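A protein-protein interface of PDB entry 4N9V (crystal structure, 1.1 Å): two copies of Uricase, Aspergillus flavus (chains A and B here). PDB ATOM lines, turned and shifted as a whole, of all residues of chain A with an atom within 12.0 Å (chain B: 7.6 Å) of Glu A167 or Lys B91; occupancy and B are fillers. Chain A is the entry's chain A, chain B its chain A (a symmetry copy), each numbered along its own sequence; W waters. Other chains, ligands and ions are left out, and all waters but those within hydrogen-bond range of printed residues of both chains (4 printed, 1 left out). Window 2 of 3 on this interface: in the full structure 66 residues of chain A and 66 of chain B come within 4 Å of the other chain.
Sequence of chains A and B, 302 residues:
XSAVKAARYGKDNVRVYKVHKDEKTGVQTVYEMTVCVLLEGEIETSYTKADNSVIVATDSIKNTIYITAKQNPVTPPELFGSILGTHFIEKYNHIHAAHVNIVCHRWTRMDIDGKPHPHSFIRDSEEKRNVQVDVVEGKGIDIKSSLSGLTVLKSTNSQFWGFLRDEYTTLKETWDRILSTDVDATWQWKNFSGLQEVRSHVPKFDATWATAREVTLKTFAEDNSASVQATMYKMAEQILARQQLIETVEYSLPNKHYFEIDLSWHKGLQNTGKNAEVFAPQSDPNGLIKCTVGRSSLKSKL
The side-chain hydroxyl of Thr A170 sits at hydrogen-bond distance from the side-chain amide nitrogen of Asn B63, 3.0 Å away.
OD2 of Asp A166 is in hydrogen-bond range of OH of Tyr B92 (2.7 Å).
The backbone carbonyl oxygen (O) of Tyr A168 is in hydrogen-bond range of the side-chain amide nitrogen (ND2) of Asn B63 (3.0 Å).
The side-chain carboxylate of Glu A167 lies within salt-bridge range of the side-chain amino group of Lys B91 (2.8 Å).
The backbone carbonyl oxygen of Ser B60 is in hydrogen-bond range of the side-chain hydroxyl of Thr B64, 2.8 Å away.
The side-chain carboxylate (OD1) of Asp A166 sits at hydrogen-bond distance from the backbone NH (N) of Tyr A168 (2.9 Å).
The backbone NH of Asp A166 lies within hydrogen-bond range of the side-chain hydroxyl of Thr A169.
Among the printed residues, merely in contact across the chains: Leu A164 with Tyr B92 (3.9 Å), Tyr A168 with Ser B60 (3.7 Å), Tyr A168 with Thr B64 (3.3 Å), Tyr A168 with Ile B67 (3.9 Å), Tyr A168 with His B87 (3.2 Å), Tyr A168 with Tyr B92 (3.8 Å) and Thr A169 with Ser B60 (3.5 Å).
Glu A167 touches just one residue of chain B: Lys B91 (2.8 Å).
His B87 touches just one residue of chain A: Tyr A168.
No residue of chain A comes within 4 Å of Ile B89.
No residue of chain A comes within 4 Å of Asn B93.
Of the printed residues of chain A, Thr B64 touches Tyr A168 (3.3 Å).
Of the printed residues of chain A, Ile B67 touches Tyr A168.
Gly B85 touches none of the printed residues of chain A.
The nearest printed residue of chain A that does not touch Lys B91 is Asp A166 (4.1 Å).
The nearest printed residue of chain B that does not touch Asp A166 is Lys B91 (4.1 Å).
Hydrophobic or aromatic side chains of chain B within 4 Å of the printed part of chain A: Ile B67, His B87 and Tyr B92.
Printed residues of chain A that touch a printed residue of chain B: Leu A164, Asp A166, Glu A167, Tyr A168, Thr A169 and Thr A170.
Hydrophobic or aromatic side chains of chain A within 4 Å of the printed part of chain B: Leu A164 and Tyr A168.
Among the printed residues, Asp or Glu carboxylates within 4 Å of a Lys or Arg side-chain nitrogen of the other chain: Glu A167 with Lys B91 (2.8 Å).
No position is printed for both chains.
Of the 11 pairs that touch across the chains among the printed residues, none has its exchanged pair printed and touching as well.
Water W2 lies within hydrogen-bond range of the backbone carbonyl oxygen (O) of Leu A164 (2.7 Å), the side-chain hydroxyl (OG) of Ser B60 (2.8 Å) and the side-chain hydroxyl (OG1) of Thr A169 (3.1 Å).
Water W1 lies within hydrogen-bond range of OE1 of Glu A167 (2.7 Å) and NZ of Lys B91 (2.9 Å).
Water W4 lies within hydrogen-bond range of OD1 of Asn B63 (2.7 Å) and OG1 of Thr A170 (3.2 Å).
Water W3 lies within hydrogen-bond range of OD1 of Asp A166 (2.8 Å), OH of Tyr B92 (2.9 Å) and OG1 of Thr A169 (3.3 Å).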
ATOM      1  N   PHE A 163      -8.971 -17.918   5.673  1.00  0.00           N
ATOM      2  CA  PHE A 163     -10.187 -17.577   4.972  1.00  0.00           C
ATOM      3  C   PHE A 163     -10.556 -18.628   3.926  1.00  0.00           C
ATOM      4  O   PHE A 163      -9.741 -19.467   3.545  1.00  0.00           O
ATOM      5  CB  PHE A 163     -10.083 -16.171   4.357  1.00  0.00           C
ATOM      6  CG  PHE A 163      -8.852 -15.963   3.522  1.00  0.00           C
ATOM      7  CD1 PHE A 163      -7.692 -15.464   4.100  1.00  0.00           C
ATOM      8  CD2 PHE A 163      -8.851 -16.268   2.172  1.00  0.00           C
ATOM      9  CE1 PHE A 163      -6.544 -15.272   3.331  1.00  0.00           C
ATOM     10  CE2 PHE A 163      -7.714 -16.062   1.407  1.00  0.00           C
ATOM     11  CZ  PHE A 163      -6.566 -15.575   1.988  1.00  0.00           C
ATOM     12  N   LEU A 164     -11.804 -18.591   3.487  1.00  0.00           N
ATOM     13  CA  LEU A 164     -12.308 -19.538   2.501  1.00  0.00           C
ATOM     14  C   LEU A 164     -11.501 -19.442   1.213  1.00  0.00           C
ATOM     15  O   LEU A 164     -11.218 -18.361   0.713  1.00  0.00           O
ATOM     16  CB  LEU A 164     -13.787 -19.255   2.234  1.00  0.00           C
ATOM     17  CG  LEU A 164     -14.545 -20.244   1.345  1.00  0.00           C
ATOM     18  CD1 LEU A 164     -16.018 -20.272   1.742  1.00  0.00           C
ATOM     19  CD2 LEU A 164     -14.384 -19.904  -0.133  1.00  0.00           C
ATOM     20  N   ARG A 165     -11.133 -20.610   0.688  1.00  0.00           N
ATOM     21  CA  ARG A 165     -10.374 -20.703  -0.556  1.00  0.00           C
ATOM     22  C   ARG A 165     -11.121 -21.575  -1.543  1.00  0.00           C
ATOM     23  O   ARG A 165     -11.362 -22.753  -1.270  1.00  0.00           O
ATOM     24  CB  ARG A 165      -8.974 -21.293  -0.330  1.00  0.00           C
ATOM     25  CG  ARG A 165      -8.164 -20.652   0.777  1.00  0.00           C
ATOM     26  CD  ARG A 165      -6.680 -21.027   0.714  1.00  0.00           C
ATOM     27  NE  ARG A 165      -6.066 -20.442  -0.466  1.00  0.00           N
ATOM     28  CZ  ARG A 165      -5.594 -19.200  -0.528  1.00  0.00           C
ATOM     29  NH1 ARG A 165      -5.588 -18.416   0.539  1.00  0.00           N
ATOM     30  NH2 ARG A 165      -5.095 -18.754  -1.665  1.00  0.00           N
ATOM     31  N   ASP A 166     -11.477 -21.013  -2.690  1.00  0.00           N
ATOM     32  CA  ASP A 166     -12.124 -21.765  -3.746  1.00  0.00           C
ATOM     33  C   ASP A 166     -11.636 -21.235  -5.095  1.00  0.00           C
ATOM     34  O   ASP A 166     -10.600 -20.555  -5.174  1.00  0.00           O
ATOM     35  CB  ASP A 166     -13.653 -21.733  -3.604  1.00  0.00           C
ATOM     36  CG  ASP A 166     -14.246 -20.353  -3.820  1.00  0.00           C
ATOM     37  OD1 ASP A 166     -13.512 -19.408  -4.202  1.00  0.00           O
ATOM     38  OD2 ASP A 166     -15.475 -20.237  -3.614  1.00  0.00           O
ATOM     39  N   GLU A 167     -12.361 -21.540  -6.162  1.00  0.00           N
ATOM     40  CA  GLU A 167     -11.909 -21.201  -7.497  1.00  0.00           C
ATOM     41  C   GLU A 167     -11.949 -19.705  -7.817  1.00  0.00           C
ATOM     42  O   GLU A 167     -11.497 -19.319  -8.891  1.00  0.00           O
ATOM     43  CB  GLU A 167     -12.685 -22.021  -8.545  1.00  0.00           C
ATOM     44  CG  GLU A 167     -14.172 -21.696  -8.692  1.00  0.00           C
ATOM     45  CD  GLU A 167     -15.112 -22.437  -7.730  1.00  0.00           C
ATOM     46  OE1 GLU A 167     -14.686 -22.897  -6.656  1.00  0.00           O
ATOM     47  OE2 GLU A 167     -16.303 -22.545  -8.067  1.00  0.00           O
ATOM     48  N   TYR A 168     -12.473 -18.889  -6.901  1.00  0.00           N
ATOM     49  CA  TYR A 168     -12.464 -17.436  -7.050  1.00  0.00           C
ATOM     50  C   TYR A 168     -11.335 -16.784  -6.269  1.00  0.00           C
ATOM     51  O   TYR A 168     -11.190 -15.559  -6.309  1.00  0.00           O
ATOM     52  CB  TYR A 168     -13.799 -16.839  -6.593  1.00  0.00           C
ATOM     53  CG  TYR A 168     -14.946 -17.336  -7.415  1.00  0.00           C
ATOM     54  CD1 TYR A 168     -15.332 -16.700  -8.579  1.00  0.00           C
ATOM     55  CD2 TYR A 168     -15.621 -18.495  -7.052  1.00  0.00           C
ATOM     56  CE1 TYR A 168     -16.378 -17.174  -9.345  1.00  0.00           C
ATOM     57  CE2 TYR A 168     -16.662 -18.974  -7.804  1.00  0.00           C
ATOM     58  CZ  TYR A 168     -17.032 -18.332  -8.957  1.00  0.00           C
ATOM     59  OH  TYR A 168     -18.069 -18.834  -9.711  1.00  0.00           O
ATOM     60  N   THR A 169     -10.541 -17.580  -5.565  1.00  0.00           N
ATOM     61  CA  THR A 169      -9.566 -17.060  -4.618  1.00  0.00           C
ATOM     62  C   THR A 169      -8.154 -17.023  -5.177  1.00  0.00           C
ATOM     63  O   THR A 169      -7.645 -18.046  -5.621  1.00  0.00           O
ATOM     64  CB  THR A 169      -9.532 -17.938  -3.352  1.00  0.00           C
ATOM     65  OG1 THR A 169     -10.856 -18.132  -2.871  1.00  0.00           O
ATOM     66  CG2 THR A 169      -8.672 -17.321  -2.261  1.00  0.00           C
ATOM     67  N   THR A 170      -7.525 -15.857  -5.134  1.00  0.00           N
ATOM     68  CA  THR A 170      -6.120 -15.709  -5.435  1.00  0.00           C
ATOM     69  C   THR A 170      -5.316 -15.172  -4.257  1.00  0.00           C
ATOM     70  O   THR A 170      -4.093 -15.272  -4.251  1.00  0.00           O
ATOM     71  CB  THR A 170      -5.907 -14.769  -6.627  1.00  0.00           C
ATOM     72  OG1 THR A 170      -6.537 -13.516  -6.355  1.00  0.00           O
ATOM     73  CG2 THR A 170      -6.494 -15.353  -7.889  1.00  0.00           C
ATOM     74  N   LEU A 171      -5.979 -14.588  -3.266  1.00  0.00           N
ATOM     75  CA  LEU A 171      -5.281 -13.931  -2.178  1.00  0.00           C
ATOM     76  C   LEU A 171      -4.420 -14.895  -1.389  1.00  0.00           C
ATOM     77  O   LEU A 171      -4.902 -15.930  -0.940  1.00  0.00           O
ATOM     78  CB  LEU A 171      -6.294 -13.269  -1.241  1.00  0.00           C
ATOM     79  CG  LEU A 171      -5.739 -12.503  -0.039  1.00  0.00           C
ATOM     80  CD1 LEU A 171      -4.950 -11.262  -0.490  1.00  0.00           C
ATOM     81  CD2 LEU A 171      -6.856 -12.081   0.897  1.00  0.00           C
ATOM     82  N   VAL B  56     -15.510 -15.203   2.799  1.00  0.00           N
ATOM     83  CA  VAL B  56     -15.167 -15.131   1.396  1.00  0.00           C
ATOM     84  C   VAL B  56     -14.356 -13.839   1.286  1.00  0.00           C
ATOM     85  O   VAL B  56     -14.879 -12.750   1.515  1.00  0.00           O
ATOM     86  CB  VAL B  56     -16.436 -15.072   0.528  1.00  0.00           C
ATOM     87  CG1 VAL B  56     -16.082 -14.870  -0.933  1.00  0.00           C
ATOM     88  CG2 VAL B  56     -17.290 -16.340   0.728  1.00  0.00           C
ATOM     89  N   SER B  60     -11.423 -11.881  -3.092  1.00  0.00           N
ATOM     90  CA  SER B  60     -12.132 -12.846  -3.920  1.00  0.00           C
ATOM     91  C   SER B  60     -13.443 -12.276  -4.442  1.00  0.00           C
ATOM     92  O   SER B  60     -13.868 -12.582  -5.558  1.00  0.00           O
ATOM     93  CB  SER B  60     -12.406 -14.127  -3.137  1.00  0.00           C
ATOM     94  OG  SER B  60     -11.201 -14.644  -2.634  1.00  0.00           O
ATOM     95  N   ASN B  63     -12.386 -10.328  -7.395  1.00  0.00           N
ATOM     96  CA  ASN B  63     -12.175 -11.216  -8.539  1.00  0.00           C
ATOM     97  C   ASN B  63     -13.508 -11.602  -9.167  1.00  0.00           C
ATOM     98  O   ASN B  63     -13.648 -11.677 -10.374  1.00  0.00           O
ATOM     99  CB  ASN B  63     -11.447 -12.495  -8.123  1.00  0.00           C
ATOM    100  CG  ASN B  63     -10.005 -12.269  -7.714  1.00  0.00           C
ATOM    101  OD1 ASN B  63      -9.376 -11.277  -8.104  1.00  0.00           O
ATOM    102  ND2 ASN B  63      -9.467 -13.199  -6.928  1.00  0.00           N
ATOM    103  N   THR B  64     -14.465 -11.921  -8.300  1.00  0.00           N
ATOM    104  CA  THR B  64     -15.772 -12.380  -8.734  1.00  0.00           C
ATOM    105  C   THR B  64     -16.527 -11.305  -9.514  1.00  0.00           C
ATOM    106  O   THR B  64     -17.225 -11.612 -10.467  1.00  0.00           O
ATOM    107  CB  THR B  64     -16.605 -12.867  -7.534  1.00  0.00           C
ATOM    108  OG1 THR B  64     -15.908 -13.923  -6.866  1.00  0.00           O
ATOM    109  CG2 THR B  64     -17.978 -13.400  -7.976  1.00  0.00           C
ATOM    110  N   ILE B  67     -14.938 -11.448 -13.016  1.00  0.00           N
ATOM    111  CA  ILE B  67     -15.324 -12.687 -13.692  1.00  0.00           C
ATOM    112  C   ILE B  67     -16.783 -12.607 -14.146  1.00  0.00           C
ATOM    113  O   ILE B  67     -17.131 -12.980 -15.270  1.00  0.00           O
ATOM    114  CB  ILE B  67     -15.091 -13.885 -12.764  1.00  0.00           C
ATOM    115  CG1 ILE B  67     -13.588 -14.140 -12.588  1.00  0.00           C
ATOM    116  CG2 ILE B  67     -15.794 -15.141 -13.303  1.00  0.00           C
ATOM    117  CD1 ILE B  67     -13.261 -14.972 -11.356  1.00  0.00           C
ATOM    118  N   GLY B  85     -25.347 -10.483  -7.306  1.00  0.00           N
ATOM    119  CA  GLY B  85     -25.816 -10.773  -5.963  1.00  0.00           C
ATOM    120  C   GLY B  85     -26.333 -12.198  -5.824  1.00  0.00           C
ATOM    121  O   GLY B  85     -26.091 -12.854  -4.815  1.00  0.00           O
ATOM    122  N   THR B  86     -27.030 -12.679  -6.847  1.00  0.00           N
ATOM    123  CA  THR B  86     -27.538 -14.049  -6.848  1.00  0.00           C
ATOM    124  C   THR B  86     -26.380 -15.043  -6.783  1.00  0.00           C
ATOM    125  O   THR B  86     -26.470 -16.056  -6.098  1.00  0.00           O
ATOM    126  CB  THR B  86     -28.405 -14.299  -8.092  1.00  0.00           C
ATOM    127  OG1 THR B  86     -29.576 -13.479  -8.025  1.00  0.00           O
ATOM    128  CG2 THR B  86     -28.824 -15.741  -8.173  1.00  0.00           C
ATOM    129  N   HIS B  87     -25.280 -14.744  -7.472  1.00  0.00           N
ATOM    130  CA  HIS B  87     -24.130 -15.611  -7.435  1.00  0.00           C
ATOM    131  C   HIS B  87     -23.667 -15.861  -6.000  1.00  0.00           C
ATOM    132  O   HIS B  87     -23.419 -16.994  -5.610  1.00  0.00           O
ATOM    133  CB  HIS B  87     -22.963 -15.048  -8.251  1.00  0.00           C
ATOM    134  CG  HIS B  87     -21.668 -15.699  -7.898  1.00  0.00           C
ATOM    135  ND1 HIS B  87     -21.305 -16.948  -8.367  1.00  0.00           N
ATOM    136  CD2 HIS B  87     -20.708 -15.327  -7.021  1.00  0.00           C
ATOM    137  CE1 HIS B  87     -20.143 -17.280  -7.836  1.00  0.00           C
ATOM    138  NE2 HIS B  87     -19.760 -16.316  -7.018  1.00  0.00           N
ATOM    139  N   PHE B  88     -23.524 -14.806  -5.209  1.00  0.00           N
ATOM    140  CA  PHE B  88     -22.972 -14.985  -3.876  1.00  0.00           C
ATOM    141  C   PHE B  88     -23.874 -15.824  -2.981  1.00  0.00           C
ATOM    142  O   PHE B  88     -23.391 -16.676  -2.231  1.00  0.00           O
ATOM    143  CB  PHE B  88     -22.637 -13.642  -3.227  1.00  0.00           C
ATOM    144  CG  PHE B  88     -21.457 -12.976  -3.857  1.00  0.00           C
ATOM    145  CD1 PHE B  88     -20.176 -13.472  -3.664  1.00  0.00           C
ATOM    146  CD2 PHE B  88     -21.621 -11.866  -4.656  1.00  0.00           C
ATOM    147  CE1 PHE B  88     -19.080 -12.865  -4.254  1.00  0.00           C
ATOM    148  CE2 PHE B  88     -20.527 -11.260  -5.256  1.00  0.00           C
ATOM    149  CZ  PHE B  88     -19.261 -11.752  -5.048  1.00  0.00           C
ATOM    150  N   ILE B  89     -25.181 -15.580  -3.023  1.00  0.00           N
ATOM    151  CA  ILE B  89     -26.063 -16.343  -2.146  1.00  0.00           C
ATOM    152  C   ILE B  89     -26.228 -17.782  -2.625  1.00  0.00           C
ATOM    153  O   ILE B  89     -26.494 -18.660  -1.828  1.00  0.00           O
ATOM    154  CB  ILE B  89     -27.445 -15.667  -1.901  1.00  0.00           C
ATOM    155  CG1 ILE B  89     -28.277 -15.553  -3.172  1.00  0.00           C
ATOM    156  CG2 ILE B  89     -27.250 -14.309  -1.227  1.00  0.00           C
ATOM    157  CD1 ILE B  89     -29.780 -15.450  -2.875  1.00  0.00           C
ATOM    158  N   GLU B  90     -26.062 -18.047  -3.911  1.00  0.00           N
ATOM    159  CA  GLU B  90     -26.183 -19.408  -4.395  1.00  0.00           C
ATOM    160  C   GLU B  90     -24.892 -20.180  -4.199  1.00  0.00           C
ATOM    161  O   GLU B  90     -24.918 -21.358  -3.890  1.00  0.00           O
ATOM    162  CB  GLU B  90     -26.589 -19.413  -5.865  1.00  0.00           C
ATOM    163  CG  GLU B  90     -28.028 -19.001  -6.061  1.00  0.00           C
ATOM    164  CD  GLU B  90     -28.507 -19.126  -7.489  1.00  0.00           C
ATOM    165  OE1 GLU B  90     -27.671 -19.320  -8.400  1.00  0.00           O
ATOM    166  OE2 GLU B  90     -29.735 -19.027  -7.703  1.00  0.00           O
ATOM    167  N   LYS B  91     -23.758 -19.533  -4.413  1.00  0.00           N
ATOM    168  CA  LYS B  91     -22.476 -20.221  -4.371  1.00  0.00           C
ATOM    169  C   LYS B  91     -22.091 -20.611  -2.951  1.00  0.00           C
ATOM    170  O   LYS B  91     -21.509 -21.664  -2.736  1.00  0.00           O
ATOM    171  CB  LYS B  91     -21.396 -19.318  -4.979  1.00  0.00           C
ATOM    172  CG  LYS B  91     -19.987 -19.916  -4.956  1.00  0.00           C
ATOM    173  CD  LYS B  91     -19.915 -21.186  -5.796  1.00  0.00           C
ATOM    174  CE  LYS B  91     -18.572 -21.870  -5.663  1.00  0.00           C
ATOM    175  NZ  LYS B  91     -18.534 -23.096  -6.510  1.00  0.00           N
ATOM    176  N   TYR B  92     -22.439 -19.767  -1.985  1.00  0.00           N
ATOM    177  CA  TYR B  92     -22.000 -19.941  -0.606  1.00  0.00           C
ATOM    178  C   TYR B  92     -23.199 -20.211   0.283  1.00  0.00           C
ATOM    179  O   TYR B  92     -24.054 -19.362   0.478  1.00  0.00           O
ATOM    180  CB  TYR B  92     -21.233 -18.707  -0.124  1.00  0.00           C
ATOM    181  CG  TYR B  92     -20.028 -18.467  -0.990  1.00  0.00           C
ATOM    182  CD1 TYR B  92     -18.928 -19.307  -0.912  1.00  0.00           C
ATOM    183  CD2 TYR B  92     -19.997 -17.430  -1.912  1.00  0.00           C
ATOM    184  CE1 TYR B  92     -17.822 -19.133  -1.736  1.00  0.00           C
ATOM    185  CE2 TYR B  92     -18.895 -17.243  -2.731  1.00  0.00           C
ATOM    186  CZ  TYR B  92     -17.818 -18.102  -2.641  1.00  0.00           C
ATOM    187  OH  TYR B  92     -16.735 -17.908  -3.464  1.00  0.00           O
ATOM    188  N   ASN B  93     -23.285 -21.426   0.803  1.00  0.00           N
ATOM    189  CA  ASN B  93     -24.443 -21.800   1.594  1.00  0.00           C
ATOM    190  C   ASN B  93     -24.694 -20.825   2.739  1.00  0.00           C
ATOM    191  O   ASN B  93     -25.839 -20.463   3.010  1.00  0.00           O
ATOM    192  CB  ASN B  93     -24.288 -23.219   2.167  1.00  0.00           C
ATOM    193  CG  ASN B  93     -24.404 -24.298   1.114  1.00  0.00           C
ATOM    194  OD1 ASN B  93     -24.787 -24.044  -0.029  1.00  0.00           O
ATOM    195  ND2 ASN B  93     -24.091 -25.524   1.505  1.00  0.00           N
ATOM    196  N   HIS B  94     -23.622 -20.388   3.395  1.00  0.00           N
ATOM    197  CA  HIS B  94     -23.737 -19.589   4.606  1.00  0.00           C
ATOM    198  C   HIS B  94     -23.892 -18.093   4.365  1.00  0.00           C
ATOM    199  O   HIS B  94     -24.065 -17.340   5.314  1.00  0.00           O
ATOM    200  CB  HIS B  94     -22.542 -19.833   5.516  1.00  0.00           C
ATOM    201  CG  HIS B  94     -21.271 -19.227   5.020  1.00  0.00           C
ATOM    202  ND1 HIS B  94     -20.618 -19.665   3.887  1.00  0.00           N
ATOM    203  CD2 HIS B  94     -20.538 -18.207   5.516  1.00  0.00           C
ATOM    204  CE1 HIS B  94     -19.532 -18.934   3.708  1.00  0.00           C
ATOM    205  NE2 HIS B  94     -19.462 -18.044   4.680  1.00  0.00           N
ATOM    206  N   ILE B  95     -23.831 -17.672   3.105  1.00  0.00           N
ATOM    207  CA  ILE B  95     -24.079 -16.282   2.754  1.00  0.00           C
ATOM    208  C   ILE B  95     -25.536 -16.166   2.372  1.00  0.00           C
ATOM    209  O   ILE B  95     -25.998 -16.871   1.497  1.00  0.00           O
ATOM    210  CB  ILE B  95     -23.167 -15.819   1.592  1.00  0.00           C
ATOM    211  CG1 ILE B  95     -21.697 -15.908   2.022  1.00  0.00           C
ATOM    212  CG2 ILE B  95     -23.545 -14.415   1.141  1.00  0.00           C
ATOM    213  CD1 ILE B  95     -21.325 -15.030   3.211  1.00  0.00           C
HETATM  214  O   HOH W   1     -16.328 -24.259  -4.969  1.00  0.00           O
HETATM  215  O   HOH W   2     -12.292 -16.341  -0.728  1.00  0.00           O
HETATM  216  O   HOH W   3     -13.999 -17.113  -2.739  1.00  0.00           O
HETATM  217  O   HOH W   4      -7.127 -10.431  -6.796  1.00  0.00           O
